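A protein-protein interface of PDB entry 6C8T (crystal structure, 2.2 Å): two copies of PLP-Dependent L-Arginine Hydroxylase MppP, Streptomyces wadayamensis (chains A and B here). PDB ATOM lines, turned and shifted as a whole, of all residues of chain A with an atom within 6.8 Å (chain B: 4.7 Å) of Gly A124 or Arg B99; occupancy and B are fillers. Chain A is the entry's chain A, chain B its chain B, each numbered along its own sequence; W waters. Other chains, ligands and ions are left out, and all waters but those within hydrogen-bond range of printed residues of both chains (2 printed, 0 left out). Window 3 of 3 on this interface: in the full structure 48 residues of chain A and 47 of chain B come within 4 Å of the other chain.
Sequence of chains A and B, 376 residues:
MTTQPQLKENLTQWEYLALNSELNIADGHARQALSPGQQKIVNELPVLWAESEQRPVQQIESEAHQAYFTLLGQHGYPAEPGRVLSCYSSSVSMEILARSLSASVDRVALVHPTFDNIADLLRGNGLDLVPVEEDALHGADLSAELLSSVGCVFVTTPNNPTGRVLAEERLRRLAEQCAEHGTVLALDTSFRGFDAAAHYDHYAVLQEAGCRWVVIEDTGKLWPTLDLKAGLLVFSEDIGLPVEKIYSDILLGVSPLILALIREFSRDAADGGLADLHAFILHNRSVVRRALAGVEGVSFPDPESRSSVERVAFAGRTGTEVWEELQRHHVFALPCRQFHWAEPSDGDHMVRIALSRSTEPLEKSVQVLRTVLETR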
ATOM      1  N   GLU A  95      18.469  25.397 -19.576  1.00  0.00           N
ATOM      2  CA  GLU A  95      18.074  24.894 -18.268  1.00  0.00           C
ATOM      3  C   GLU A  95      19.281  24.321 -17.546  1.00  0.00           C
ATOM      4  O   GLU A  95      19.443  24.519 -16.333  1.00  0.00           O
ATOM      5  CB  GLU A  95      16.982  23.838 -18.417  1.00  0.00           C
ATOM      6  CG  GLU A  95      16.584  23.105 -17.124  1.00  0.00           C
ATOM      7  CD  GLU A  95      15.732  23.930 -16.196  1.00  0.00           C
ATOM      8  OE1 GLU A  95      15.480  25.119 -16.495  1.00  0.00           O
ATOM      9  OE2 GLU A  95      15.292  23.390 -15.150  1.00  0.00           O
ATOM     10  N   ALA A  98      21.334  27.385 -16.412  1.00  0.00           N
ATOM     11  CA  ALA A  98      20.703  28.099 -15.306  1.00  0.00           C
ATOM     12  C   ALA A  98      20.849  27.319 -14.006  1.00  0.00           C
ATOM     13  O   ALA A  98      21.235  27.877 -12.981  1.00  0.00           O
ATOM     14  CB  ALA A  98      19.234  28.375 -15.607  1.00  0.00           C
ATOM     15  N   ARG A  99      20.580  26.010 -14.035  1.00  0.00           N
ATOM     16  CA  ARG A  99      20.745  25.226 -12.817  1.00  0.00           C
ATOM     17  C   ARG A  99      22.189  25.188 -12.377  1.00  0.00           C
ATOM     18  O   ARG A  99      22.460  25.182 -11.186  1.00  0.00           O
ATOM     19  CB  ARG A  99      20.231  23.809 -13.024  1.00  0.00           C
ATOM     20  CG  ARG A  99      18.767  23.712 -12.719  1.00  0.00           C
ATOM     21  CD  ARG A  99      18.488  22.744 -11.604  1.00  0.00           C
ATOM     22  NE  ARG A  99      18.268  21.450 -12.220  1.00  0.00           N
ATOM     23  CZ  ARG A  99      18.997  20.380 -12.018  1.00  0.00           C
ATOM     24  NH1 ARG A  99      20.027  20.421 -11.168  1.00  0.00           N
ATOM     25  NH2 ARG A  99      18.680  19.276 -12.688  1.00  0.00           N
ATOM     26  N   ALA A 119      15.243  34.710 -19.646  1.00  0.00           N
ATOM     27  CA  ALA A 119      15.001  35.298 -18.337  1.00  0.00           C
ATOM     28  C   ALA A 119      14.209  34.357 -17.448  1.00  0.00           C
ATOM     29  O   ALA A 119      14.509  34.228 -16.260  1.00  0.00           O
ATOM     30  CB  ALA A 119      14.281  36.642 -18.491  1.00  0.00           C
ATOM     31  N   ASP A 120      13.192  33.693 -17.995  1.00  0.00           N
ATOM     32  CA  ASP A 120      12.324  32.862 -17.152  1.00  0.00           C
ATOM     33  C   ASP A 120      13.031  31.591 -16.670  1.00  0.00           C
ATOM     34  O   ASP A 120      12.737  31.080 -15.582  1.00  0.00           O
ATOM     35  CB  ASP A 120      11.046  32.504 -17.919  1.00  0.00           C
ATOM     36  CG  ASP A 120      10.120  33.706 -18.129  1.00  0.00           C
ATOM     37  OD1 ASP A 120      10.273  34.714 -17.424  1.00  0.00           O
ATOM     38  OD2 ASP A 120       9.236  33.635 -18.995  1.00  0.00           O
ATOM     39  N   LEU A 121      13.936  31.040 -17.470  1.00  0.00           N
ATOM     40  CA  LEU A 121      14.681  29.888 -16.998  1.00  0.00           C
ATOM     41  C   LEU A 121      15.699  30.290 -15.951  1.00  0.00           C
ATOM     42  O   LEU A 121      15.922  29.545 -14.997  1.00  0.00           O
ATOM     43  CB  LEU A 121      15.344  29.174 -18.158  1.00  0.00           C
ATOM     44  CG  LEU A 121      14.430  28.439 -19.138  1.00  0.00           C
ATOM     45  CD1 LEU A 121      15.233  27.884 -20.316  1.00  0.00           C
ATOM     46  CD2 LEU A 121      13.714  27.284 -18.466  1.00  0.00           C
ATOM     47  N   LEU A 122      16.280  31.479 -16.069  1.00  0.00           N
ATOM     48  CA  LEU A 122      17.206  31.930 -15.041  1.00  0.00           C
ATOM     49  C   LEU A 122      16.456  32.231 -13.747  1.00  0.00           C
ATOM     50  O   LEU A 122      16.824  31.743 -12.670  1.00  0.00           O
ATOM     51  CB  LEU A 122      17.976  33.157 -15.543  1.00  0.00           C
ATOM     52  CG  LEU A 122      19.034  32.858 -16.614  1.00  0.00           C
ATOM     53  CD1 LEU A 122      19.496  34.173 -17.298  1.00  0.00           C
ATOM     54  CD2 LEU A 122      20.254  32.069 -16.056  1.00  0.00           C
ATOM     55  N   ARG A 123      15.380  33.020 -13.838  1.00  0.00           N
ATOM     56  CA  ARG A 123      14.618  33.353 -12.643  1.00  0.00           C
ATOM     57  C   ARG A 123      14.039  32.110 -12.019  1.00  0.00           C
ATOM     58  O   ARG A 123      13.999  31.998 -10.794  1.00  0.00           O
ATOM     59  CB  ARG A 123      13.477  34.302 -12.955  1.00  0.00           C
ATOM     60  CG  ARG A 123      13.870  35.717 -13.281  1.00  0.00           C
ATOM     61  CD  ARG A 123      12.742  36.621 -12.869  1.00  0.00           C
ATOM     62  NE  ARG A 123      12.689  37.854 -13.642  1.00  0.00           N
ATOM     63  CZ  ARG A 123      12.126  37.955 -14.840  1.00  0.00           C
ATOM     64  NH1 ARG A 123      11.581  36.888 -15.419  1.00  0.00           N
ATOM     65  NH2 ARG A 123      12.117  39.126 -15.460  1.00  0.00           N
ATOM     66  N   GLY A 124      13.532  31.191 -12.848  1.00  0.00           N
ATOM     67  CA  GLY A 124      12.926  29.980 -12.322  1.00  0.00           C
ATOM     68  C   GLY A 124      13.908  29.163 -11.503  1.00  0.00           C
ATOM     69  O   GLY A 124      13.514  28.428 -10.594  1.00  0.00           O
ATOM     70  N   ASN A 125      15.191  29.287 -11.805  1.00  0.00           N
ATOM     71  CA  ASN A 125      16.220  28.557 -11.091  1.00  0.00           C
ATOM     72  C   ASN A 125      16.870  29.398 -10.019  1.00  0.00           C
ATOM     73  O   ASN A 125      17.919  29.024  -9.498  1.00  0.00           O
ATOM     74  CB  ASN A 125      17.246  28.033 -12.067  1.00  0.00           C
ATOM     75  CG  ASN A 125      16.744  26.761 -12.779  1.00  0.00           C
ATOM     76  OD1 ASN A 125      16.631  25.705 -12.169  1.00  0.00           O
ATOM     77  ND2 ASN A 125      16.367  26.895 -14.033  1.00  0.00           N
ATOM     78  N   GLY A 126      16.237  30.507  -9.657  1.00  0.00           N
ATOM     79  CA  GLY A 126      16.578  31.229  -8.466  1.00  0.00           C
ATOM     80  C   GLY A 126      17.552  32.360  -8.680  1.00  0.00           C
ATOM     81  O   GLY A 126      18.003  32.956  -7.705  1.00  0.00           O
ATOM     82  N   LEU A 127      17.866  32.692  -9.918  1.00  0.00           N
ATOM     83  CA  LEU A 127      18.801  33.765 -10.199  1.00  0.00           C
ATOM     84  C   LEU A 127      18.079  35.106 -10.294  1.00  0.00           C
ATOM     85  O   LEU A 127      17.028  35.206 -10.916  1.00  0.00           O
ATOM     86  CB  LEU A 127      19.535  33.458 -11.504  1.00  0.00           C
ATOM     87  CG  LEU A 127      20.395  32.230 -11.201  1.00  0.00           C
ATOM     88  CD1 LEU A 127      20.217  31.187 -12.232  1.00  0.00           C
ATOM     89  CD2 LEU A 127      21.848  32.595 -10.984  1.00  0.00           C
ATOM     90  N   GLU B  95      12.702  16.666 -15.025  1.00  0.00           N
ATOM     91  CA  GLU B  95      13.214  17.990 -14.658  1.00  0.00           C
ATOM     92  C   GLU B  95      12.074  18.964 -14.447  1.00  0.00           C
ATOM     93  O   GLU B  95      12.056  19.698 -13.453  1.00  0.00           O
ATOM     94  CB  GLU B  95      14.171  18.518 -15.733  1.00  0.00           C
ATOM     95  CG  GLU B  95      14.606  19.946 -15.580  1.00  0.00           C
ATOM     96  CD  GLU B  95      15.609  20.137 -14.447  1.00  0.00           C
ATOM     97  OE1 GLU B  95      15.897  19.150 -13.758  1.00  0.00           O
ATOM     98  OE2 GLU B  95      16.109  21.258 -14.242  1.00  0.00           O
ATOM     99  N   ILE B  96      11.099  18.975 -15.363  1.00  0.00           N
ATOM    100  CA  ILE B  96       9.922  19.838 -15.202  1.00  0.00           C
ATOM    101  C   ILE B  96       9.208  19.548 -13.873  1.00  0.00           C
ATOM    102  O   ILE B  96       8.949  20.453 -13.071  1.00  0.00           O
ATOM    103  CB  ILE B  96       8.982  19.672 -16.407  1.00  0.00           C
ATOM    104  CG1 ILE B  96       9.636  20.226 -17.663  1.00  0.00           C
ATOM    105  CG2 ILE B  96       7.641  20.402 -16.168  1.00  0.00           C
ATOM    106  CD1 ILE B  96       8.995  19.771 -18.940  1.00  0.00           C
ATOM    107  N   LEU B  97       8.894  18.282 -13.610  1.00  0.00           N
ATOM    108  CA  LEU B  97       8.222  17.918 -12.360  1.00  0.00           C
ATOM    109  C   LEU B  97       9.051  18.314 -11.152  1.00  0.00           C
ATOM    110  O   LEU B  97       8.527  18.856 -10.166  1.00  0.00           O
ATOM    111  CB  LEU B  97       7.955  16.410 -12.317  1.00  0.00           C
ATOM    112  CG  LEU B  97       7.407  15.873 -10.988  1.00  0.00           C
ATOM    113  CD1 LEU B  97       6.071  16.513 -10.737  1.00  0.00           C
ATOM    114  CD2 LEU B  97       7.270  14.328 -11.005  1.00  0.00           C
ATOM    115  N   ALA B  98      10.347  17.996 -11.187  1.00  0.00           N
ATOM    116  CA  ALA B  98      11.207  18.290 -10.050  1.00  0.00           C
ATOM    117  C   ALA B  98      11.188  19.779  -9.746  1.00  0.00           C
ATOM    118  O   ALA B  98      10.877  20.188  -8.627  1.00  0.00           O
ATOM    119  CB  ALA B  98      12.627  17.818 -10.316  1.00  0.00           C
ATOM    120  N   ARG B  99      11.482  20.612 -10.747  1.00  0.00           N
ATOM    121  CA  ARG B  99      11.488  22.039 -10.494  1.00  0.00           C
ATOM    122  C   ARG B  99      10.090  22.518 -10.103  1.00  0.00           C
ATOM    123  O   ARG B  99       9.958  23.415  -9.291  1.00  0.00           O
ATOM    124  CB  ARG B  99      12.041  22.796 -11.715  1.00  0.00           C
ATOM    125  CG  ARG B  99      12.348  24.240 -11.381  1.00  0.00           C
ATOM    126  CD  ARG B  99      13.612  24.734 -12.060  1.00  0.00           C
ATOM    127  NE  ARG B  99      13.506  24.938 -13.494  1.00  0.00           N
ATOM    128  CZ  ARG B  99      12.736  25.848 -14.066  1.00  0.00           C
ATOM    129  NH1 ARG B  99      12.772  25.948 -15.378  1.00  0.00           N
ATOM    130  NH2 ARG B  99      11.933  26.642 -13.343  1.00  0.00           N
ATOM    131  N   SER B 100       9.038  21.881 -10.622  1.00  0.00           N
ATOM    132  CA  SER B 100       7.687  22.251 -10.234  1.00  0.00           C
ATOM    133  C   SER B 100       7.426  21.906  -8.779  1.00  0.00           C
ATOM    134  O   SER B 100       6.814  22.687  -8.058  1.00  0.00           O
ATOM    135  CB  SER B 100       6.659  21.543 -11.107  1.00  0.00           C
ATOM    136  OG  SER B 100       6.650  22.068 -12.425  1.00  0.00           O
ATOM    137  N   LEU B 101       7.876  20.736  -8.339  1.00  0.00           N
ATOM    138  CA  LEU B 101       7.697  20.329  -6.956  1.00  0.00           C
ATOM    139  C   LEU B 101       8.391  21.277  -6.003  1.00  0.00           C
ATOM    140  O   LEU B 101       7.889  21.534  -4.903  1.00  0.00           O
ATOM    141  CB  LEU B 101       8.244  18.927  -6.740  1.00  0.00           C
ATOM    142  CG  LEU B 101       7.405  17.749  -7.220  1.00  0.00           C
ATOM    143  CD1 LEU B 101       8.238  16.469  -7.265  1.00  0.00           C
ATOM    144  CD2 LEU B 101       6.182  17.601  -6.284  1.00  0.00           C
ATOM    145  N   SER B 102       9.576  21.763  -6.378  1.00  0.00           N
ATOM    146  CA  SER B 102      10.320  22.616  -5.479  1.00  0.00           C
ATOM    147  C   SER B 102       9.608  23.939  -5.216  1.00  0.00           C
ATOM    148  O   SER B 102       9.983  24.622  -4.272  1.00  0.00           O
ATOM    149  CB  SER B 102      11.731  22.884  -6.036  1.00  0.00           C
ATOM    150  OG  SER B 102      11.676  23.817  -7.087  1.00  0.00           O
ATOM    151  N   ALA B 103       8.587  24.300  -6.005  1.00  0.00           N
ATOM    152  CA  ALA B 103       7.811  25.502  -5.708  1.00  0.00           C
ATOM    153  C   ALA B 103       7.020  25.366  -4.410  1.00  0.00           C
ATOM    154  O   ALA B 103       6.776  26.375  -3.747  1.00  0.00           O
ATOM    155  CB  ALA B 103       6.856  25.834  -6.859  1.00  0.00           C
ATOM    156  N   ASN B 125      17.177  19.971  -7.676  1.00  0.00           N
ATOM    157  CA  ASN B 125      16.181  21.023  -7.591  1.00  0.00           C
ATOM    158  C   ASN B 125      15.789  21.356  -6.147  1.00  0.00           C
ATOM    159  O   ASN B 125      14.758  21.982  -5.912  1.00  0.00           O
ATOM    160  CB  ASN B 125      14.982  20.624  -8.428  1.00  0.00           C
ATOM    161  CG  ASN B 125      15.222  20.870  -9.913  1.00  0.00           C
ATOM    162  OD1 ASN B 125      15.057  21.980 -10.367  1.00  0.00           O
ATOM    163  ND2 ASN B 125      15.621  19.837 -10.668  1.00  0.00           N
ATOM    164  N   ILE B 246       6.183  25.689 -16.366  1.00  0.00           N
ATOM    165  CA  ILE B 246       7.599  25.383 -16.537  1.00  0.00           C
ATOM    166  C   ILE B 246       7.820  24.597 -17.818  1.00  0.00           C
ATOM    167  O   ILE B 246       8.812  24.804 -18.523  1.00  0.00           O
ATOM    168  CB  ILE B 246       8.148  24.665 -15.301  1.00  0.00           C
ATOM    169  CG1 ILE B 246       8.187  25.651 -14.124  1.00  0.00           C
ATOM    170  CG2 ILE B 246       9.566  24.168 -15.559  1.00  0.00           C
ATOM    171  CD1 ILE B 246       8.510  25.006 -12.780  1.00  0.00           C
ATOM    172  N   ILE B 250      10.291  25.648 -21.178  1.00  0.00           N
ATOM    173  CA  ILE B 250      11.330  24.817 -21.798  1.00  0.00           C
ATOM    174  C   ILE B 250      11.030  24.514 -23.258  1.00  0.00           C
ATOM    175  O   ILE B 250      11.947  24.504 -24.082  1.00  0.00           O
ATOM    176  CB  ILE B 250      11.533  23.532 -20.985  1.00  0.00           C
ATOM    177  CG1 ILE B 250      12.160  23.900 -19.639  1.00  0.00           C
ATOM    178  CG2 ILE B 250      12.481  22.604 -21.679  1.00  0.00           C
ATOM    179  CD1 ILE B 250      12.192  22.805 -18.705  1.00  0.00           C
HETATM  180  O   HOH W   1      10.564  27.517 -11.074  1.00  0.00           O
HETATM  181  O   HOH W   2      11.406  28.533 -15.555  1.00  0.00           O
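The guanidinium group (NE) of Arg A99 sits close to the side-chain amide nitrogen (ND2) of Asn B125, at 3.5 Å.
OE2 of Glu B95 lies within salt-bridge range of NE of Arg A99 (3.0 Å).
The side-chain amide oxygen (OD1) of Asn A125 lies close to the guanidinium group (NE) of Arg B99, 3.5 Å away.
OE2 of Glu A95 is in salt-bridge range of NE of Arg B99 (2.9 Å).
The side-chain carboxylate (OE2) of Glu A95 lies close to the side-chain carboxylate (OE2) of Glu B95.
The side-chain amide nitrogen (ND2) of Asn B125 lies within hydrogen-bond range of the side-chain carboxylate (OE1) of Glu B95 (3.2 Å).
O of Arg B99 sits at hydrogen-bond distance from OG of Ser B102 (2.8 Å).
The backbone carbonyl oxygen (O) of Leu A121 sits at hydrogen-bond distance from the side-chain amide nitrogen (ND2) of Asn A125, at 2.9 Å.
The side-chain carboxylate of Glu A95 lies within hydrogen-bond range of the side-chain amide nitrogen of Asn A125, at 3.2 Å.
Leu A121 touches Arg B99.
Leu A121 touches Ile B250.
Arg B99 touches Gly A124.
Of the printed residues of chain B, Leu A121 touches Arg B99 and Ile B250.
Printed residues of chain A within 4 Å of Arg B99: Glu A95 (2.9 Å), Leu A121 (3.5 Å), Gly A124 (3.6 Å) and Asn A125 (3.2 Å).
Of the printed residues of chain A, Asn B125 touches Arg A99 (3.5 Å).
The nearest printed residue of chain B that does not touch Gly A124 is Ser B102 (6.1 Å).
The nearest residue of chain A that does not touch Arg B99 is Asp A120 (5.0 Å).
The nearest printed residue of chain B that does not touch Glu A95 is Ile B250 (4.5 Å).
Of the 12 printed residues of chain A, 5 touch a printed residue of chain B.
Hydrophobic or aromatic side chains of chain A that line the printed part of chain B: Leu A121.
Of the 12 printed residues of chain B, 4 touch a printed residue of chain A.
Among the printed residues, Asp or Glu carboxylates within 4 Å of a Lys or Arg side-chain nitrogen of the other chain: Glu A95 with Arg B99 (2.9 Å) and Arg A99 with Glu B95 (3.0 Å).
Glu A95 touches its own counterpart, Glu B95.
Glu A95 touches Arg B99, and with the chains exchanged Arg A99 touches Glu B95.
Arg A99 touches Asn B125, and with the chains exchanged Asn A125 touches Arg B99.
Positions printed for both chains: 95, 98, 99 and 125.
Of the 8 pairs that touch across the chains among the printed residues, 5 have their exchanged pair printed and touching as well.
Water W1 lies within hydrogen-bond range of the guanidinium group of Arg B99 and the backbone carbonyl oxygen of Gly A124.
Water W2 lies within hydrogen-bond range of O of Asp A120 (2.9 Å) and NH1 of Arg B99 (2.9 Å).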
